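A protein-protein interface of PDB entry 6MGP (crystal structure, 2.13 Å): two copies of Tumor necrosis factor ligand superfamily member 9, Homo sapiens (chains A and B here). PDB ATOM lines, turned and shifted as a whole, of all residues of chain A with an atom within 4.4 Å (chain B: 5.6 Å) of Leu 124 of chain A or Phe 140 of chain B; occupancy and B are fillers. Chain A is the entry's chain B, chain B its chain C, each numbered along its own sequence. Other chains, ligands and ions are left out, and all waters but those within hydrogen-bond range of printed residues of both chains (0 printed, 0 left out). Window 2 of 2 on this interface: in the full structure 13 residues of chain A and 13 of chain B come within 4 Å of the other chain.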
ATOM      1  N   PHE A  88     -15.161  16.016   2.590  1.00  0.00           N
ATOM      2  CA  PHE A  88     -14.418  16.725   1.561  1.00  0.00           C
ATOM      3  C   PHE A  88     -15.400  17.368   0.592  1.00  0.00           C
ATOM      4  O   PHE A  88     -16.583  17.021   0.538  1.00  0.00           O
ATOM      5  CB  PHE A  88     -13.358  15.840   0.840  1.00  0.00           C
ATOM      6  CG  PHE A  88     -13.886  14.593   0.141  1.00  0.00           C
ATOM      7  CD1 PHE A  88     -15.239  14.332  -0.011  1.00  0.00           C
ATOM      8  CD2 PHE A  88     -12.980  13.676  -0.378  1.00  0.00           C
ATOM      9  CE1 PHE A  88     -15.679  13.182  -0.663  1.00  0.00           C
ATOM     10  CE2 PHE A  88     -13.411  12.523  -1.034  1.00  0.00           C
ATOM     11  CZ  PHE A  88     -14.762  12.280  -1.180  1.00  0.00           C
ATOM     12  N   VAL A 104     -16.655  14.403 -12.887  1.00  0.00           N
ATOM     13  CA  VAL A 104     -15.435  14.301 -12.104  1.00  0.00           C
ATOM     14  C   VAL A 104     -15.802  13.744 -10.737  1.00  0.00           C
ATOM     15  O   VAL A 104     -16.805  14.159 -10.143  1.00  0.00           O
ATOM     16  CB  VAL A 104     -14.747  15.674 -11.978  1.00  0.00           C
ATOM     17  CG1 VAL A 104     -13.674  15.630 -10.925  1.00  0.00           C
ATOM     18  CG2 VAL A 104     -14.167  16.091 -13.319  1.00  0.00           C
ATOM     19  N   SER A 105     -15.007  12.794 -10.242  1.00  0.00           N
ATOM     20  CA  SER A 105     -15.277  12.160  -8.957  1.00  0.00           C
ATOM     21  C   SER A 105     -14.056  12.221  -8.050  1.00  0.00           C
ATOM     22  O   SER A 105     -12.913  12.257  -8.516  1.00  0.00           O
ATOM     23  CB  SER A 105     -15.706  10.702  -9.132  1.00  0.00           C
ATOM     24  OG  SER A 105     -14.607   9.909  -9.526  1.00  0.00           O
ATOM     25  N   LEU A 106     -14.321  12.231  -6.741  1.00  0.00           N
ATOM     26  CA  LEU A 106     -13.310  12.159  -5.693  1.00  0.00           C
ATOM     27  C   LEU A 106     -13.559  10.918  -4.848  1.00  0.00           C
ATOM     28  O   LEU A 106     -14.703  10.630  -4.480  1.00  0.00           O
ATOM     29  CB  LEU A 106     -13.356  13.382  -4.777  1.00  0.00           C
ATOM     30  CG  LEU A 106     -12.637  14.680  -5.114  1.00  0.00           C
ATOM     31  CD1 LEU A 106     -12.634  15.549  -3.877  1.00  0.00           C
ATOM     32  CD2 LEU A 106     -11.225  14.438  -5.594  1.00  0.00           C
ATOM     33  N   ALA A 123     -16.899   9.022  -1.158  1.00  0.00           N
ATOM     34  CA  ALA A 123     -16.893   9.104  -2.611  1.00  0.00           C
ATOM     35  C   ALA A 123     -17.926  10.123  -3.047  1.00  0.00           C
ATOM     36  O   ALA A 123     -19.014  10.204  -2.469  1.00  0.00           O
ATOM     37  CB  ALA A 123     -17.177   7.735  -3.257  1.00  0.00           C
ATOM     38  N   LEU A 124     -17.588  10.902  -4.070  1.00  0.00           N
ATOM     39  CA  LEU A 124     -18.499  11.944  -4.525  1.00  0.00           C
ATOM     40  C   LEU A 124     -18.246  12.219  -6.001  1.00  0.00           C
ATOM     41  O   LEU A 124     -17.092  12.340  -6.419  1.00  0.00           O
ATOM     42  CB  LEU A 124     -18.297  13.194  -3.673  1.00  0.00           C
ATOM     43  CG  LEU A 124     -18.795  14.545  -4.138  1.00  0.00           C
ATOM     44  CD1 LEU A 124     -20.280  14.681  -3.831  1.00  0.00           C
ATOM     45  CD2 LEU A 124     -17.981  15.591  -3.410  1.00  0.00           C
ATOM     46  N   THR A 125     -19.315  12.283  -6.793  1.00  0.00           N
ATOM     47  CA  THR A 125     -19.221  12.639  -8.204  1.00  0.00           C
ATOM     48  C   THR A 125     -19.965  13.948  -8.442  1.00  0.00           C
ATOM     49  O   THR A 125     -21.046  14.165  -7.885  1.00  0.00           O
ATOM     50  CB  THR A 125     -19.798  11.525  -9.106  1.00  0.00           C
ATOM     51  OG1 THR A 125     -19.070  10.308  -8.904  1.00  0.00           O
ATOM     52  CG2 THR A 125     -19.709  11.914 -10.584  1.00  0.00           C
ATOM     53  N   VAL A 126     -19.374  14.826  -9.252  1.00  0.00           N
ATOM     54  CA  VAL A 126     -20.031  16.043  -9.712  1.00  0.00           C
ATOM     55  C   VAL A 126     -20.047  16.044 -11.238  1.00  0.00           C
ATOM     56  O   VAL A 126     -19.126  15.535 -11.887  1.00  0.00           O
ATOM     57  CB  VAL A 126     -19.341  17.309  -9.161  1.00  0.00           C
ATOM     58  CG1 VAL A 126     -19.033  17.141  -7.677  1.00  0.00           C
ATOM     59  CG2 VAL A 126     -18.086  17.579  -9.912  1.00  0.00           C
ATOM     60  N   GLY A 141     -19.691  19.768  -5.168  1.00  0.00           N
ATOM     61  CA  GLY A 141     -20.222  18.672  -4.378  1.00  0.00           C
ATOM     62  C   GLY A 141     -19.584  18.667  -3.004  1.00  0.00           C
ATOM     63  O   GLY A 141     -18.476  19.177  -2.813  1.00  0.00           O
ATOM     64  N   PHE A 142     -20.299  18.074  -2.043  1.00  0.00           N
ATOM     65  CA  PHE A 142     -19.837  17.958  -0.662  1.00  0.00           C
ATOM     66  C   PHE A 142     -20.328  16.634  -0.089  1.00  0.00           C
ATOM     67  O   PHE A 142     -21.505  16.300  -0.242  1.00  0.00           O
ATOM     68  CB  PHE A 142     -20.358  19.129   0.194  1.00  0.00           C
ATOM     69  CG  PHE A 142     -20.063  18.996   1.667  1.00  0.00           C
ATOM     70  CD1 PHE A 142     -20.910  18.283   2.499  1.00  0.00           C
ATOM     71  CD2 PHE A 142     -18.938  19.600   2.220  1.00  0.00           C
ATOM     72  CE1 PHE A 142     -20.627  18.157   3.852  1.00  0.00           C
ATOM     73  CE2 PHE A 142     -18.658  19.480   3.566  1.00  0.00           C
ATOM     74  CZ  PHE A 142     -19.503  18.755   4.380  1.00  0.00           C
ATOM     75  N   GLN A 143     -19.444  15.904   0.604  1.00  0.00           N
ATOM     76  CA  GLN A 143     -19.862  14.733   1.370  1.00  0.00           C
ATOM     77  C   GLN A 143     -19.151  14.667   2.722  1.00  0.00           C
ATOM     78  O   GLN A 143     -17.981  15.041   2.842  1.00  0.00           O
ATOM     79  CB  GLN A 143     -19.608  13.430   0.600  1.00  0.00           C
ATOM     80  CG  GLN A 143     -20.206  12.197   1.271  1.00  0.00           C
ATOM     81  CD  GLN A 143     -19.819  10.907   0.577  1.00  0.00           C
ATOM     82  OE1 GLN A 143     -18.635  10.576   0.466  1.00  0.00           O
ATOM     83  NE2 GLN A 143     -20.817  10.166   0.108  1.00  0.00           N
ATOM     84  N   GLN B  89     -27.369  11.214   4.291  1.00  0.00           N
ATOM     85  CA  GLN B  89     -26.783  11.099   2.971  1.00  0.00           C
ATOM     86  C   GLN B  89     -27.693  10.212   2.142  1.00  0.00           C
ATOM     87  O   GLN B  89     -28.233   9.224   2.652  1.00  0.00           O
ATOM     88  CB  GLN B  89     -25.371  10.516   3.090  1.00  0.00           C
ATOM     89  CG  GLN B  89     -24.680  10.175   1.811  1.00  0.00           C
ATOM     90  CD  GLN B  89     -23.331   9.536   2.068  1.00  0.00           C
ATOM     91  OE1 GLN B  89     -22.591   9.957   2.962  1.00  0.00           O
ATOM     92  NE2 GLN B  89     -23.003   8.510   1.285  1.00  0.00           N
ATOM     93  N   LEU B  90     -27.895  10.585   0.876  1.00  0.00           N
ATOM     94  CA  LEU B  90     -28.791   9.863  -0.024  1.00  0.00           C
ATOM     95  C   LEU B  90     -28.073   9.629  -1.344  1.00  0.00           C
ATOM     96  O   LEU B  90     -27.746  10.586  -2.053  1.00  0.00           O
ATOM     97  CB  LEU B  90     -30.092  10.642  -0.248  1.00  0.00           C
ATOM     98  CG  LEU B  90     -31.090  10.029  -1.232  1.00  0.00           C
ATOM     99  CD1 LEU B  90     -31.353   8.576  -0.879  1.00  0.00           C
ATOM    100  CD2 LEU B  90     -32.391  10.819  -1.230  1.00  0.00           C
ATOM    101  N   GLU B  91     -27.819   8.365  -1.666  1.00  0.00           N
ATOM    102  CA  GLU B  91     -27.171   8.003  -2.915  1.00  0.00           C
ATOM    103  C   GLU B  91     -27.990   6.928  -3.612  1.00  0.00           C
ATOM    104  O   GLU B  91     -28.414   5.954  -2.978  1.00  0.00           O
ATOM    105  CB  GLU B  91     -25.743   7.515  -2.683  1.00  0.00           C
ATOM    106  CG  GLU B  91     -24.978   7.246  -3.975  1.00  0.00           C
ATOM    107  CD  GLU B  91     -23.492   7.087  -3.736  1.00  0.00           C
ATOM    108  OE1 GLU B  91     -22.811   6.486  -4.595  1.00  0.00           O
ATOM    109  OE2 GLU B  91     -23.005   7.564  -2.684  1.00  0.00           O
ATOM    110  N   LEU B  92     -28.219   7.113  -4.910  1.00  0.00           N
ATOM    111  CA  LEU B  92     -28.979   6.170  -5.716  1.00  0.00           C
ATOM    112  C   LEU B  92     -28.170   5.788  -6.944  1.00  0.00           C
ATOM    113  O   LEU B  92     -27.303   6.543  -7.393  1.00  0.00           O
ATOM    114  CB  LEU B  92     -30.335   6.753  -6.126  1.00  0.00           C
ATOM    115  CG  LEU B  92     -31.166   7.256  -4.943  1.00  0.00           C
ATOM    116  CD1 LEU B  92     -31.027   8.760  -4.806  1.00  0.00           C
ATOM    117  CD2 LEU B  92     -32.630   6.848  -5.092  1.00  0.00           C
ATOM    118  N   VAL B 126     -33.281  14.484  -3.841  1.00  0.00           N
ATOM    119  CA  VAL B 126     -32.290  14.177  -4.862  1.00  0.00           C
ATOM    120  C   VAL B 126     -33.021  13.915  -6.169  1.00  0.00           C
ATOM    121  O   VAL B 126     -33.927  13.073  -6.224  1.00  0.00           O
ATOM    122  CB  VAL B 126     -31.429  12.965  -4.467  1.00  0.00           C
ATOM    123  CG1 VAL B 126     -30.525  12.593  -5.610  1.00  0.00           C
ATOM    124  CG2 VAL B 126     -30.621  13.275  -3.224  1.00  0.00           C
ATOM    125  N   ARG B 136     -25.180  10.415 -16.159  1.00  0.00           N
ATOM    126  CA  ARG B 136     -24.625   9.303 -15.403  1.00  0.00           C
ATOM    127  C   ARG B 136     -25.740   8.528 -14.721  1.00  0.00           C
ATOM    128  O   ARG B 136     -26.915   8.903 -14.756  1.00  0.00           O
ATOM    129  CB  ARG B 136     -23.604   9.752 -14.369  1.00  0.00           C
ATOM    130  CG  ARG B 136     -23.957  10.938 -13.522  1.00  0.00           C
ATOM    131  CD  ARG B 136     -22.727  11.321 -12.736  1.00  0.00           C
ATOM    132  NE  ARG B 136     -23.037  12.366 -11.775  1.00  0.00           N
ATOM    133  CZ  ARG B 136     -23.557  12.154 -10.575  1.00  0.00           C
ATOM    134  NH1 ARG B 136     -23.805  10.919 -10.167  1.00  0.00           N
ATOM    135  NH2 ARG B 136     -23.811  13.186  -9.779  1.00  0.00           N
ATOM    136  N   SER B 138     -25.887   7.608 -11.370  1.00  0.00           N
ATOM    137  CA  SER B 138     -25.920   7.733  -9.927  1.00  0.00           C
ATOM    138  C   SER B 138     -26.331   9.152  -9.579  1.00  0.00           C
ATOM    139  O   SER B 138     -26.194  10.077 -10.386  1.00  0.00           O
ATOM    140  CB  SER B 138     -24.572   7.375  -9.294  1.00  0.00           C
ATOM    141  OG  SER B 138     -23.570   8.296  -9.688  1.00  0.00           O
ATOM    142  N   ALA B 139     -26.853   9.307  -8.371  1.00  0.00           N
ATOM    143  CA  ALA B 139     -27.300  10.596  -7.878  1.00  0.00           C
ATOM    144  C   ALA B 139     -26.994  10.676  -6.388  1.00  0.00           C
ATOM    145  O   ALA B 139     -26.991   9.661  -5.684  1.00  0.00           O
ATOM    146  CB  ALA B 139     -28.794  10.807  -8.149  1.00  0.00           C
ATOM    147  N   PHE B 140     -26.727  11.887  -5.911  1.00  0.00           N
ATOM    148  CA  PHE B 140     -26.258  12.048  -4.542  1.00  0.00           C
ATOM    149  C   PHE B 140     -26.775  13.359  -3.963  1.00  0.00           C
ATOM    150  O   PHE B 140     -26.908  14.365  -4.668  1.00  0.00           O
ATOM    151  CB  PHE B 140     -24.725  11.992  -4.476  1.00  0.00           C
ATOM    152  CG  PHE B 140     -24.163  12.462  -3.172  1.00  0.00           C
ATOM    153  CD1 PHE B 140     -24.044  11.591  -2.099  1.00  0.00           C
ATOM    154  CD2 PHE B 140     -23.754  13.778  -3.013  1.00  0.00           C
ATOM    155  CE1 PHE B 140     -23.529  12.026  -0.882  1.00  0.00           C
ATOM    156  CE2 PHE B 140     -23.243  14.218  -1.805  1.00  0.00           C
ATOM    157  CZ  PHE B 140     -23.127  13.340  -0.738  1.00  0.00           C
ATOM    158  N   GLY B 141     -27.066  13.330  -2.666  1.00  0.00           N
ATOM    159  CA  GLY B 141     -27.406  14.519  -1.904  1.00  0.00           C
ATOM    160  C   GLY B 141     -26.983  14.385  -0.451  1.00  0.00           C
ATOM    161  O   GLY B 141     -27.046  13.288   0.115  1.00  0.00           O
ATOM    162  N   PHE B 142     -26.536  15.485   0.157  1.00  0.00           N
ATOM    163  CA  PHE B 142     -26.124  15.513   1.555  1.00  0.00           C
ATOM    164  C   PHE B 142     -26.718  16.746   2.223  1.00  0.00           C
ATOM    165  O   PHE B 142     -26.746  17.823   1.620  1.00  0.00           O
ATOM    166  CB  PHE B 142     -24.585  15.528   1.686  1.00  0.00           C
ATOM    167  CG  PHE B 142     -24.093  15.596   3.112  1.00  0.00           C
ATOM    168  CD1 PHE B 142     -23.996  16.813   3.778  1.00  0.00           C
ATOM    169  CD2 PHE B 142     -23.720  14.441   3.787  1.00  0.00           C
ATOM    170  CE1 PHE B 142     -23.557  16.871   5.088  1.00  0.00           C
ATOM    171  CE2 PHE B 142     -23.273  14.498   5.093  1.00  0.00           C
ATOM    172  CZ  PHE B 142     -23.191  15.716   5.743  1.00  0.00           C
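NH2 of Arg 136 of chain B is in hydrogen-bond range of O of Thr 125 of chain A. NE2 of Gln 89 of chain B sits close to NE2 of Gln 143 of chain A.
The backbone carbonyl oxygen (O) of Gln 143 of chain A is in hydrogen-bond range of the backbone NH (N) of Phe 88 of chain A (3.0 Å). The backbone NH (N) of Leu 106 of chain A is in hydrogen-bond range of the backbone carbonyl oxygen (O) of Leu 124 of chain A (2.8 Å). N of Ala 123 of chain A sits at hydrogen-bond distance from OE1 of Gln 143 of chain A. The guanidinium group of Arg 136 of chain B is in hydrogen-bond range of the backbone carbonyl oxygen of Ser 138 of chain B (2.5 Å).
Leu 124 of chain A touches Phe 140 of chain B. Phe 140 of chain B touches Phe 142 of chain A. CE1 of Phe 142 of chain B touches CE1 of Phe 142 of chain A (3.4 Å). Phe 140 of chain B touches Gln 143 of chain A (CE1 to NE2, 3.4 Å).
Of chain B, only Phe 140 (3.6 Å) comes within 4 Å of Leu 124 of chain A. Phe 140 of chain B touches just these residues of chain A: Leu 124 (3.6 Å), Phe 142 (3.1 Å) and Gln 143 (3.4 Å). Printed residues of chain B within 4 Å of Gln 143 of chain A: Gln 89 (3.0 Å) and Phe 140 (3.4 Å). Of the printed residues of chain A, Arg 136 of chain B touches Thr 125. Ser 138 of chain B touches none of the printed residues of chain A. Gly 141 of chain A touches none of the printed residues of chain B. The nearest printed residue of chain B that does not touch Leu 124 of chain A is Glu 91 of chain B (6.5 Å). The nearest printed residue of chain A that does not touch Phe 140 of chain B is Ala 123 of chain A (5.1 Å).
Printed residues of chain B that touch a printed residue of chain A: Gln 89, Arg 136, Phe 140 and Phe 142. Of the 11 printed residues of chain A, 4 touch a printed residue of chain B. Hydrophobic or aromatic side chains of chain A within 4 Å of the printed part of chain B: Leu 124 and Phe 142. Among the printed residues, 6 pairs touch across the chains.
Phe 142 of chain A touches its own counterpart, Phe 142 of chain B. Of the 6 pairs that touch across the chains among the printed residues, 1 has its exchanged pair printed and touching as well.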
